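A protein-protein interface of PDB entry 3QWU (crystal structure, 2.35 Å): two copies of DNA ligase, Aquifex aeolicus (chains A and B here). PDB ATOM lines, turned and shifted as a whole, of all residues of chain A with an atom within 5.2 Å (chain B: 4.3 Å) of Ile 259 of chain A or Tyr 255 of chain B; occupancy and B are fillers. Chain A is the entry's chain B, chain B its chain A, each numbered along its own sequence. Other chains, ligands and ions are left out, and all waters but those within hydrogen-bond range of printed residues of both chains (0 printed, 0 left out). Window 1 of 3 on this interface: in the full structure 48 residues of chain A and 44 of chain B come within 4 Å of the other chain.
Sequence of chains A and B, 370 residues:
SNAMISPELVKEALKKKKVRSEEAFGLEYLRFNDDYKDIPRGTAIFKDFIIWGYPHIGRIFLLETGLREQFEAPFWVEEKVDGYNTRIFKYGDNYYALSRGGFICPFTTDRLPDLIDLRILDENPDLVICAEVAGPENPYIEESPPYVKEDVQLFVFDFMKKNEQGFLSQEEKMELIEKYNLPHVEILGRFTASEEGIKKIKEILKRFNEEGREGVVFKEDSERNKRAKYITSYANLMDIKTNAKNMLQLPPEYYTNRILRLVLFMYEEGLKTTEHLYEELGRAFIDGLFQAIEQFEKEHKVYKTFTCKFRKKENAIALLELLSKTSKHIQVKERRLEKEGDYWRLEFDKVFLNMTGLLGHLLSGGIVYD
Tyr 255 of chain B touches its own counterpart, Tyr 255 of chain A. Thr 256 of chain A touches Tyr 255 of chain B, but with the chains exchanged Tyr 255 of chain A does not touch Thr 256 of chain B (6.0 Å). Ile 259 of chain A touches Tyr 255 of chain B, but with the chains exchanged Tyr 255 of chain A does not touch Ile 259 of chain B (6.5 Å). Phe 285 of chain B touches its own counterpart, Phe 285 of chain A. Positions printed for both chains: 253, 255, 256, 257, 258, 259 and 285. Of the 11 pairs that touch across the chains among the printed residues, 4 have their exchanged pair printed and touching as well.
OH of Tyr 255 of chain B sits close to N of Thr 256 of chain A (2.9 Å).
Tyr 255 of chain B touches Met 247 of chain A (CB to CE, 3.4 Å). CE of Met 247 of chain A touches N of Thr 256 of chain B, 3.2 Å away. O of Leu 250 of chain B touches CG of Pro 252 of chain A, at 3.6 Å. Pro 252 of chain A touches Tyr 255 of chain B. CB of Tyr 255 of chain A touches CZ of Tyr 255 of chain B, 3.5 Å away. CE2 of Tyr 255 of chain B touches CD1 of Ile 259 of chain A (3.9 Å). CD1 of Ile 259 of chain A touches CD1 of Phe 285 of chain B, at 3.2 Å. Leu 289 of chain B touches Ile 259 of chain A (CD2 to CG2, 3.7 Å). CD1 of Phe 285 of chain A touches CD1 of Ile 259 of chain B (3.9 Å). Phe 285 of chain A touches Phe 285 of chain B.
Hydrophobic or aromatic side chains of chain A within 4 Å of the printed part of chain B: Met 247, Pro 252, Tyr 255, Ile 259 and Phe 285. Hydrophobic or aromatic side chains of chain B that line the printed part of chain A: Tyr 255, Ile 259, Phe 285 and Leu 289. Among the printed residues, 11 pairs touch across the chains. Among the printed residues, no Asp or Glu carboxylate lies within 4 Å of a Lys or Arg side-chain nitrogen of the other chain.
Ile 259 of chain A touches just these residues of chain B: Tyr 255, Phe 285 and Leu 289. Of the printed residues of chain B, Phe 285 of chain A touches Ile 259 and Phe 285. Tyr 255 of chain B touches just these residues of chain A: Met 247 (3.4 Å), Pro 252 (3.2 Å), Tyr 255 (3.5 Å), Thr 256 (2.8 Å) and Ile 259 (3.9 Å). Printed residues of chain A within 4 Å of Thr 256 of chain B: Met 247. The nearest printed residue of chain B that does not touch Phe 285 of chain A is Tyr 255 of chain B (4.5 Å).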
ATOM      1  N   ILE A 240     -18.639  21.480 -19.533  1.00  0.00           N
ATOM      2  CA  ILE A 240     -17.938  20.270 -19.160  1.00  0.00           C
ATOM      3  C   ILE A 240     -16.807  20.010 -20.172  1.00  0.00           C
ATOM      4  O   ILE A 240     -15.654  20.029 -19.814  1.00  0.00           O
ATOM      5  CB  ILE A 240     -18.907  19.036 -19.016  1.00  0.00           C
ATOM      6  CG1 ILE A 240     -19.874  19.274 -17.853  1.00  0.00           C
ATOM      7  CG2 ILE A 240     -18.109  17.774 -18.823  1.00  0.00           C
ATOM      8  CD1 ILE A 240     -20.906  18.162 -17.579  1.00  0.00           C
ATOM      9  N   MET A 247      -9.386  20.226 -15.621  1.00  0.00           N
ATOM     10  CA  MET A 247      -9.877  19.385 -14.533  1.00  0.00           C
ATOM     11  C   MET A 247      -9.095  19.478 -13.227  1.00  0.00           C
ATOM     12  O   MET A 247      -9.687  19.368 -12.163  1.00  0.00           O
ATOM     13  CB  MET A 247      -9.939  17.907 -14.955  1.00  0.00           C
ATOM     14  CG  MET A 247     -11.032  17.598 -16.009  1.00  0.00           C
ATOM     15  SD  MET A 247     -11.601  15.895 -15.988  1.00  0.00           S
ATOM     16  CE  MET A 247     -12.457  15.937 -14.440  1.00  0.00           C
ATOM     17  N   PRO A 252     -14.227  19.762  -7.280  1.00  0.00           N
ATOM     18  CA  PRO A 252     -15.173  18.763  -7.797  1.00  0.00           C
ATOM     19  C   PRO A 252     -16.592  19.377  -7.975  1.00  0.00           C
ATOM     20  O   PRO A 252     -17.226  19.146  -9.022  1.00  0.00           O
ATOM     21  CB  PRO A 252     -15.100  17.603  -6.775  1.00  0.00           C
ATOM     22  CG  PRO A 252     -14.303  18.117  -5.595  1.00  0.00           C
ATOM     23  CD  PRO A 252     -13.478  19.279  -6.102  1.00  0.00           C
ATOM     24  N   GLU A 253     -17.025  20.223  -7.022  1.00  0.00           N
ATOM     25  CA  GLU A 253     -18.332  20.918  -7.093  1.00  0.00           C
ATOM     26  C   GLU A 253     -18.631  21.431  -8.499  1.00  0.00           C
ATOM     27  O   GLU A 253     -19.758  21.318  -8.953  1.00  0.00           O
ATOM     28  CB  GLU A 253     -18.433  22.084  -6.110  1.00  0.00           C
ATOM     29  CG  GLU A 253     -18.134  21.721  -4.652  1.00  0.00           C
ATOM     30  CD  GLU A 253     -16.633  21.538  -4.383  1.00  0.00           C
ATOM     31  OE1 GLU A 253     -15.838  22.439  -4.729  1.00  0.00           O
ATOM     32  OE2 GLU A 253     -16.257  20.485  -3.844  1.00  0.00           O
ATOM     33  N   TYR A 255     -18.305  20.196 -11.255  1.00  0.00           N
ATOM     34  CA  TYR A 255     -18.828  19.195 -12.180  1.00  0.00           C
ATOM     35  C   TYR A 255     -20.165  18.622 -11.716  1.00  0.00           C
ATOM     36  O   TYR A 255     -21.085  18.482 -12.519  1.00  0.00           O
ATOM     37  CB  TYR A 255     -17.774  18.106 -12.440  1.00  0.00           C
ATOM     38  CG  TYR A 255     -16.645  18.609 -13.292  1.00  0.00           C
ATOM     39  CD1 TYR A 255     -16.869  19.006 -14.611  1.00  0.00           C
ATOM     40  CD2 TYR A 255     -15.362  18.699 -12.792  1.00  0.00           C
ATOM     41  CE1 TYR A 255     -15.840  19.477 -15.422  1.00  0.00           C
ATOM     42  CE2 TYR A 255     -14.313  19.165 -13.590  1.00  0.00           C
ATOM     43  CZ  TYR A 255     -14.562  19.554 -14.916  1.00  0.00           C
ATOM     44  OH  TYR A 255     -13.521  20.045 -15.690  1.00  0.00           O
ATOM     45  N   THR A 256     -20.269  18.324 -10.425  1.00  0.00           N
ATOM     46  CA  THR A 256     -21.517  17.804  -9.815  1.00  0.00           C
ATOM     47  C   THR A 256     -22.681  18.825  -9.791  1.00  0.00           C
ATOM     48  O   THR A 256     -23.853  18.498  -9.541  1.00  0.00           O
ATOM     49  CB  THR A 256     -21.216  17.349  -8.380  1.00  0.00           C
ATOM     50  OG1 THR A 256     -22.284  17.738  -7.501  1.00  0.00           O
ATOM     51  CG2 THR A 256     -19.878  17.927  -7.921  1.00  0.00           C
ATOM     52  N   ASN A 257     -22.330  20.078 -10.014  1.00  0.00           N
ATOM     53  CA  ASN A 257     -23.270  21.158 -10.095  1.00  0.00           C
ATOM     54  C   ASN A 257     -23.843  21.138 -11.509  1.00  0.00           C
ATOM     55  O   ASN A 257     -25.045  21.187 -11.710  1.00  0.00           O
ATOM     56  CB  ASN A 257     -22.499  22.432  -9.795  1.00  0.00           C
ATOM     57  CG  ASN A 257     -23.332  23.613  -9.797  1.00  0.00           C
ATOM     58  OD1 ASN A 257     -23.664  24.190 -10.871  1.00  0.00           O
ATOM     59  ND2 ASN A 257     -23.688  24.045  -8.591  1.00  0.00           N
ATOM     60  N   ARG A 258     -22.950  21.019 -12.485  1.00  0.00           N
ATOM     61  CA  ARG A 258     -23.359  20.951 -13.879  1.00  0.00           C
ATOM     62  C   ARG A 258     -24.000  19.631 -14.193  1.00  0.00           C
ATOM     63  O   ARG A 258     -24.841  19.593 -15.067  1.00  0.00           O
ATOM     64  CB  ARG A 258     -22.203  21.244 -14.841  1.00  0.00           C
ATOM     65  CG  ARG A 258     -21.437  22.523 -14.451  1.00  0.00           C
ATOM     66  CD  ARG A 258     -20.934  23.339 -15.596  1.00  0.00           C
ATOM     67  NE  ARG A 258     -20.851  24.795 -15.351  1.00  0.00           N
ATOM     68  CZ  ARG A 258     -20.425  25.417 -14.241  1.00  0.00           C
ATOM     69  NH1 ARG A 258     -19.963  24.755 -13.155  1.00  0.00           N
ATOM     70  NH2 ARG A 258     -20.440  26.764 -14.227  1.00  0.00           N
ATOM     71  N   ILE A 259     -23.655  18.554 -13.484  1.00  0.00           N
ATOM     72  CA  ILE A 259     -24.363  17.292 -13.694  1.00  0.00           C
ATOM     73  C   ILE A 259     -25.791  17.395 -13.219  1.00  0.00           C
ATOM     74  O   ILE A 259     -26.731  16.969 -13.896  1.00  0.00           O
ATOM     75  CB  ILE A 259     -23.680  16.091 -13.009  1.00  0.00           C
ATOM     76  CG1 ILE A 259     -22.305  15.839 -13.644  1.00  0.00           C
ATOM     77  CG2 ILE A 259     -24.509  14.797 -13.214  1.00  0.00           C
ATOM     78  CD1 ILE A 259     -21.560  14.751 -12.910  1.00  0.00           C
ATOM     79  N   LEU A 260     -25.951  17.955 -12.031  1.00  0.00           N
ATOM     80  CA  LEU A 260     -27.253  18.223 -11.491  1.00  0.00           C
ATOM     81  C   LEU A 260     -28.119  19.084 -12.383  1.00  0.00           C
ATOM     82  O   LEU A 260     -29.335  18.910 -12.387  1.00  0.00           O
ATOM     83  CB  LEU A 260     -27.110  18.956 -10.178  1.00  0.00           C
ATOM     84  CG  LEU A 260     -26.816  18.073  -9.001  1.00  0.00           C
ATOM     85  CD1 LEU A 260     -26.148  18.929  -7.849  1.00  0.00           C
ATOM     86  CD2 LEU A 260     -28.129  17.428  -8.664  1.00  0.00           C
ATOM     87  N   ARG A 261     -27.522  20.061 -13.055  1.00  0.00           N
ATOM     88  CA  ARG A 261     -28.272  20.904 -13.949  1.00  0.00           C
ATOM     89  C   ARG A 261     -28.828  20.077 -15.078  1.00  0.00           C
ATOM     90  O   ARG A 261     -29.940  20.284 -15.510  1.00  0.00           O
ATOM     91  CB  ARG A 261     -27.368  21.983 -14.567  1.00  0.00           C
ATOM     92  CG  ARG A 261     -27.052  23.178 -13.642  1.00  0.00           C
ATOM     93  CD  ARG A 261     -26.027  24.094 -14.314  1.00  0.00           C
ATOM     94  NE  ARG A 261     -25.122  24.735 -13.365  1.00  0.00           N
ATOM     95  CZ  ARG A 261     -24.188  25.617 -13.726  1.00  0.00           C
ATOM     96  NH1 ARG A 261     -23.364  26.136 -12.813  1.00  0.00           N
ATOM     97  NH2 ARG A 261     -24.057  25.970 -15.004  1.00  0.00           N
ATOM     98  N   LEU A 262     -28.004  19.167 -15.591  1.00  0.00           N
ATOM     99  CA  LEU A 262     -28.415  18.332 -16.640  1.00  0.00           C
ATOM    100  C   LEU A 262     -29.494  17.387 -16.138  1.00  0.00           C
ATOM    101  O   LEU A 262     -30.536  17.266 -16.773  1.00  0.00           O
ATOM    102  CB  LEU A 262     -27.209  17.575 -17.197  1.00  0.00           C
ATOM    103  CG  LEU A 262     -26.284  18.442 -18.073  1.00  0.00           C
ATOM    104  CD1 LEU A 262     -25.002  17.666 -18.434  1.00  0.00           C
ATOM    105  CD2 LEU A 262     -26.987  18.946 -19.373  1.00  0.00           C
ATOM    106  N   VAL A 263     -29.235  16.706 -15.019  1.00  0.00           N
ATOM    107  CA  VAL A 263     -30.182  15.763 -14.441  1.00  0.00           C
ATOM    108  C   VAL A 263     -31.535  16.403 -14.054  1.00  0.00           C
ATOM    109  O   VAL A 263     -32.567  15.782 -14.227  1.00  0.00           O
ATOM    110  CB  VAL A 263     -29.600  15.001 -13.189  1.00  0.00           C
ATOM    111  CG1 VAL A 263     -30.667  14.015 -12.597  1.00  0.00           C
ATOM    112  CG2 VAL A 263     -28.297  14.210 -13.541  1.00  0.00           C
ATOM    113  N   LEU A 264     -31.542  17.634 -13.568  1.00  0.00           N
ATOM    114  CA  LEU A 264     -32.795  18.248 -13.189  1.00  0.00           C
ATOM    115  C   LEU A 264     -33.606  18.651 -14.402  1.00  0.00           C
ATOM    116  O   LEU A 264     -34.790  18.570 -14.357  1.00  0.00           O
ATOM    117  CB  LEU A 264     -32.587  19.420 -12.206  1.00  0.00           C
ATOM    118  CG  LEU A 264     -32.217  18.803 -10.851  1.00  0.00           C
ATOM    119  CD1 LEU A 264     -31.667  19.794  -9.879  1.00  0.00           C
ATOM    120  CD2 LEU A 264     -33.453  18.166 -10.283  1.00  0.00           C
ATOM    121  N   LEU A 281     -23.379  13.561 -22.434  1.00  0.00           N
ATOM    122  CA  LEU A 281     -22.619  13.803 -21.167  1.00  0.00           C
ATOM    123  C   LEU A 281     -21.314  12.986 -21.156  1.00  0.00           C
ATOM    124  O   LEU A 281     -20.249  13.468 -20.719  1.00  0.00           O
ATOM    125  CB  LEU A 281     -23.459  13.488 -19.936  1.00  0.00           C
ATOM    126  CG  LEU A 281     -22.748  13.606 -18.574  1.00  0.00           C
ATOM    127  CD1 LEU A 281     -22.135  14.941 -18.333  1.00  0.00           C
ATOM    128  CD2 LEU A 281     -23.718  13.171 -17.450  1.00  0.00           C
ATOM    129  N   PHE A 285     -17.211  14.605 -21.142  1.00  0.00           N
ATOM    130  CA  PHE A 285     -16.012  14.283 -20.369  1.00  0.00           C
ATOM    131  C   PHE A 285     -14.994  13.599 -21.224  1.00  0.00           C
ATOM    132  O   PHE A 285     -13.826  13.984 -21.224  1.00  0.00           O
ATOM    133  CB  PHE A 285     -16.322  13.368 -19.219  1.00  0.00           C
ATOM    134  CG  PHE A 285     -17.045  14.019 -18.116  1.00  0.00           C
ATOM    135  CD1 PHE A 285     -16.408  14.987 -17.316  1.00  0.00           C
ATOM    136  CD2 PHE A 285     -18.344  13.685 -17.823  1.00  0.00           C
ATOM    137  CE1 PHE A 285     -17.063  15.561 -16.264  1.00  0.00           C
ATOM    138  CE2 PHE A 285     -19.035  14.344 -16.775  1.00  0.00           C
ATOM    139  CZ  PHE A 285     -18.386  15.245 -15.996  1.00  0.00           C
ATOM    140  N   LEU B 250     -17.455  14.569  -1.820  1.00  0.00           N
ATOM    141  CA  LEU B 250     -16.490  14.114  -2.840  1.00  0.00           C
ATOM    142  C   LEU B 250     -15.098  14.686  -2.712  1.00  0.00           C
ATOM    143  O   LEU B 250     -14.928  15.895  -2.800  1.00  0.00           O
ATOM    144  CB  LEU B 250     -16.945  14.509  -4.244  1.00  0.00           C
ATOM    145  CG  LEU B 250     -18.035  13.731  -4.980  1.00  0.00           C
ATOM    146  CD1 LEU B 250     -18.278  14.414  -6.346  1.00  0.00           C
ATOM    147  CD2 LEU B 250     -17.729  12.238  -5.129  1.00  0.00           C
ATOM    148  N   GLU B 253     -10.518  15.022  -6.180  1.00  0.00           N
ATOM    149  CA  GLU B 253     -10.259  14.467  -7.510  1.00  0.00           C
ATOM    150  C   GLU B 253     -11.085  13.229  -7.809  1.00  0.00           C
ATOM    151  O   GLU B 253     -10.568  12.343  -8.441  1.00  0.00           O
ATOM    152  CB  GLU B 253      -8.771  14.066  -7.682  1.00  0.00           C
ATOM    153  CG  GLU B 253      -7.680  15.136  -7.492  1.00  0.00           C
ATOM    154  CD  GLU B 253      -6.272  14.642  -7.896  1.00  0.00           C
ATOM    155  OE1 GLU B 253      -6.148  13.490  -8.406  1.00  0.00           O
ATOM    156  OE2 GLU B 253      -5.294  15.414  -7.712  1.00  0.00           O
ATOM    157  N   TYR B 254     -12.334  13.101  -7.374  1.00  0.00           N
ATOM    158  CA  TYR B 254     -13.119  11.943  -7.875  1.00  0.00           C
ATOM    159  C   TYR B 254     -13.291  12.085  -9.429  1.00  0.00           C
ATOM    160  O   TYR B 254     -13.241  11.084 -10.144  1.00  0.00           O
ATOM    161  CB  TYR B 254     -14.480  11.785  -7.149  1.00  0.00           C
ATOM    162  CG  TYR B 254     -14.816  10.384  -6.616  1.00  0.00           C
ATOM    163  CD1 TYR B 254     -14.183   9.853  -5.475  1.00  0.00           C
ATOM    164  CD2 TYR B 254     -15.806   9.607  -7.218  1.00  0.00           C
ATOM    165  CE1 TYR B 254     -14.515   8.536  -4.957  1.00  0.00           C
ATOM    166  CE2 TYR B 254     -16.136   8.304  -6.735  1.00  0.00           C
ATOM    167  CZ  TYR B 254     -15.492   7.768  -5.606  1.00  0.00           C
ATOM    168  OH  TYR B 254     -15.858   6.486  -5.171  1.00  0.00           O
ATOM    169  N   TYR B 255     -13.428  13.324  -9.946  1.00  0.00           N
ATOM    170  CA  TYR B 255     -13.734  13.517 -11.373  1.00  0.00           C
ATOM    171  C   TYR B 255     -12.545  13.164 -12.180  1.00  0.00           C
ATOM    172  O   TYR B 255     -12.536  12.143 -12.878  1.00  0.00           O
ATOM    173  CB  TYR B 255     -14.203  14.965 -11.738  1.00  0.00           C
ATOM    174  CG  TYR B 255     -15.582  15.185 -11.246  1.00  0.00           C
ATOM    175  CD1 TYR B 255     -15.807  15.904 -10.079  1.00  0.00           C
ATOM    176  CD2 TYR B 255     -16.670  14.596 -11.894  1.00  0.00           C
ATOM    177  CE1 TYR B 255     -17.059  16.041  -9.573  1.00  0.00           C
ATOM    178  CE2 TYR B 255     -17.943  14.745 -11.409  1.00  0.00           C
ATOM    179  CZ  TYR B 255     -18.128  15.475 -10.234  1.00  0.00           C
ATOM    180  OH  TYR B 255     -19.377  15.632  -9.694  1.00  0.00           O
ATOM    181  N   THR B 256     -11.543  14.024 -12.090  1.00  0.00           N
ATOM    182  CA  THR B 256     -10.327  13.826 -12.820  1.00  0.00           C
ATOM    183  C   THR B 256      -9.814  12.334 -12.753  1.00  0.00           C
ATOM    184  O   THR B 256      -9.185  11.833 -13.704  1.00  0.00           O
ATOM    185  CB  THR B 256      -9.258  14.873 -12.360  1.00  0.00           C
ATOM    186  OG1 THR B 256      -7.934  14.408 -12.668  1.00  0.00           O
ATOM    187  CG2 THR B 256      -9.362  15.197 -10.840  1.00  0.00           C
ATOM    188  N   ASN B 257     -10.131  11.631 -11.656  1.00  0.00           N
ATOM    189  CA  ASN B 257      -9.525  10.350 -11.362  1.00  0.00           C
ATOM    190  C   ASN B 257     -10.269   9.168 -11.929  1.00  0.00           C
ATOM    191  O   ASN B 257      -9.681   8.368 -12.624  1.00  0.00           O
ATOM    192  CB  ASN B 257      -9.353  10.175  -9.861  1.00  0.00           C
ATOM    193  CG  ASN B 257      -8.269   9.226  -9.538  1.00  0.00           C
ATOM    194  OD1 ASN B 257      -8.481   8.013  -9.476  1.00  0.00           O
ATOM    195  ND2 ASN B 257      -7.055   9.767  -9.365  1.00  0.00           N
ATOM    196  N   ARG B 258     -11.554   9.041 -11.629  1.00  0.00           N
ATOM    197  CA  ARG B 258     -12.300   7.893 -12.164  1.00  0.00           C
ATOM    198  C   ARG B 258     -12.592   7.987 -13.677  1.00  0.00           C
ATOM    199  O   ARG B 258     -12.647   6.983 -14.371  1.00  0.00           O
ATOM    200  CB  ARG B 258     -13.526   7.604 -11.314  1.00  0.00           C
ATOM    201  CG  ARG B 258     -13.219   6.548 -10.197  1.00  0.00           C
ATOM    202  CD  ARG B 258     -14.258   6.504  -9.122  1.00  0.00           C
ATOM    203  NE  ARG B 258     -13.793   5.727  -7.969  1.00  0.00           N
ATOM    204  CZ  ARG B 258     -13.010   6.188  -6.999  1.00  0.00           C
ATOM    205  NH1 ARG B 258     -12.585   7.457  -6.984  1.00  0.00           N
ATOM    206  NH2 ARG B 258     -12.646   5.354  -6.026  1.00  0.00           N
ATOM    207  N   ILE B 259     -12.686   9.216 -14.179  1.00  0.00           N
ATOM    208  CA  ILE B 259     -12.844   9.464 -15.591  1.00  0.00           C
ATOM    209  C   ILE B 259     -11.563   9.179 -16.355  1.00  0.00           C
ATOM    210  O   ILE B 259     -11.600   8.533 -17.400  1.00  0.00           O
ATOM    211  CB  ILE B 259     -13.311  10.923 -15.854  1.00  0.00           C
ATOM    212  CG1 ILE B 259     -14.726  11.086 -15.295  1.00  0.00           C
ATOM    213  CG2 ILE B 259     -13.279  11.220 -17.317  1.00  0.00           C
ATOM    214  CD1 ILE B 259     -15.025  12.454 -14.753  1.00  0.00           C
ATOM    215  N   PHE B 285     -23.559   8.624 -14.182  1.00  0.00           N
ATOM    216  CA  PHE B 285     -23.877   9.842 -13.445  1.00  0.00           C
ATOM    217  C   PHE B 285     -25.364  10.109 -13.426  1.00  0.00           C
ATOM    218  O   PHE B 285     -25.944  10.432 -12.402  1.00  0.00           O
ATOM    219  CB  PHE B 285     -23.241  11.062 -14.067  1.00  0.00           C
ATOM    220  CG  PHE B 285     -21.757  11.185 -13.832  1.00  0.00           C
ATOM    221  CD1 PHE B 285     -21.260  11.556 -12.587  1.00  0.00           C
ATOM    222  CD2 PHE B 285     -20.876  11.002 -14.845  1.00  0.00           C
ATOM    223  CE1 PHE B 285     -19.923  11.699 -12.375  1.00  0.00           C
ATOM    224  CE2 PHE B 285     -19.528  11.115 -14.601  1.00  0.00           C
ATOM    225  CZ  PHE B 285     -19.072  11.494 -13.365  1.00  0.00           C
ATOM    226  N   LEU B 289     -28.203   9.632  -9.942  1.00  0.00           N
ATOM    227  CA  LEU B 289     -28.776  10.868  -9.437  1.00  0.00           C
ATOM    228  C   LEU B 289     -30.283  10.859  -9.655  1.00  0.00           C
ATOM    229  O   LEU B 289     -31.006  11.276  -8.786  1.00  0.00           O
ATOM    230  CB  LEU B 289     -28.090  12.091 -10.114  1.00  0.00           C
ATOM    231  CG  LEU B 289     -27.340  13.154  -9.306  1.00  0.00           C
ATOM    232  CD1 LEU B 289     -26.950  12.765  -7.851  1.00  0.00           C
ATOM    233  CD2 LEU B 289     -26.135  13.664 -10.047  1.00  0.00           C
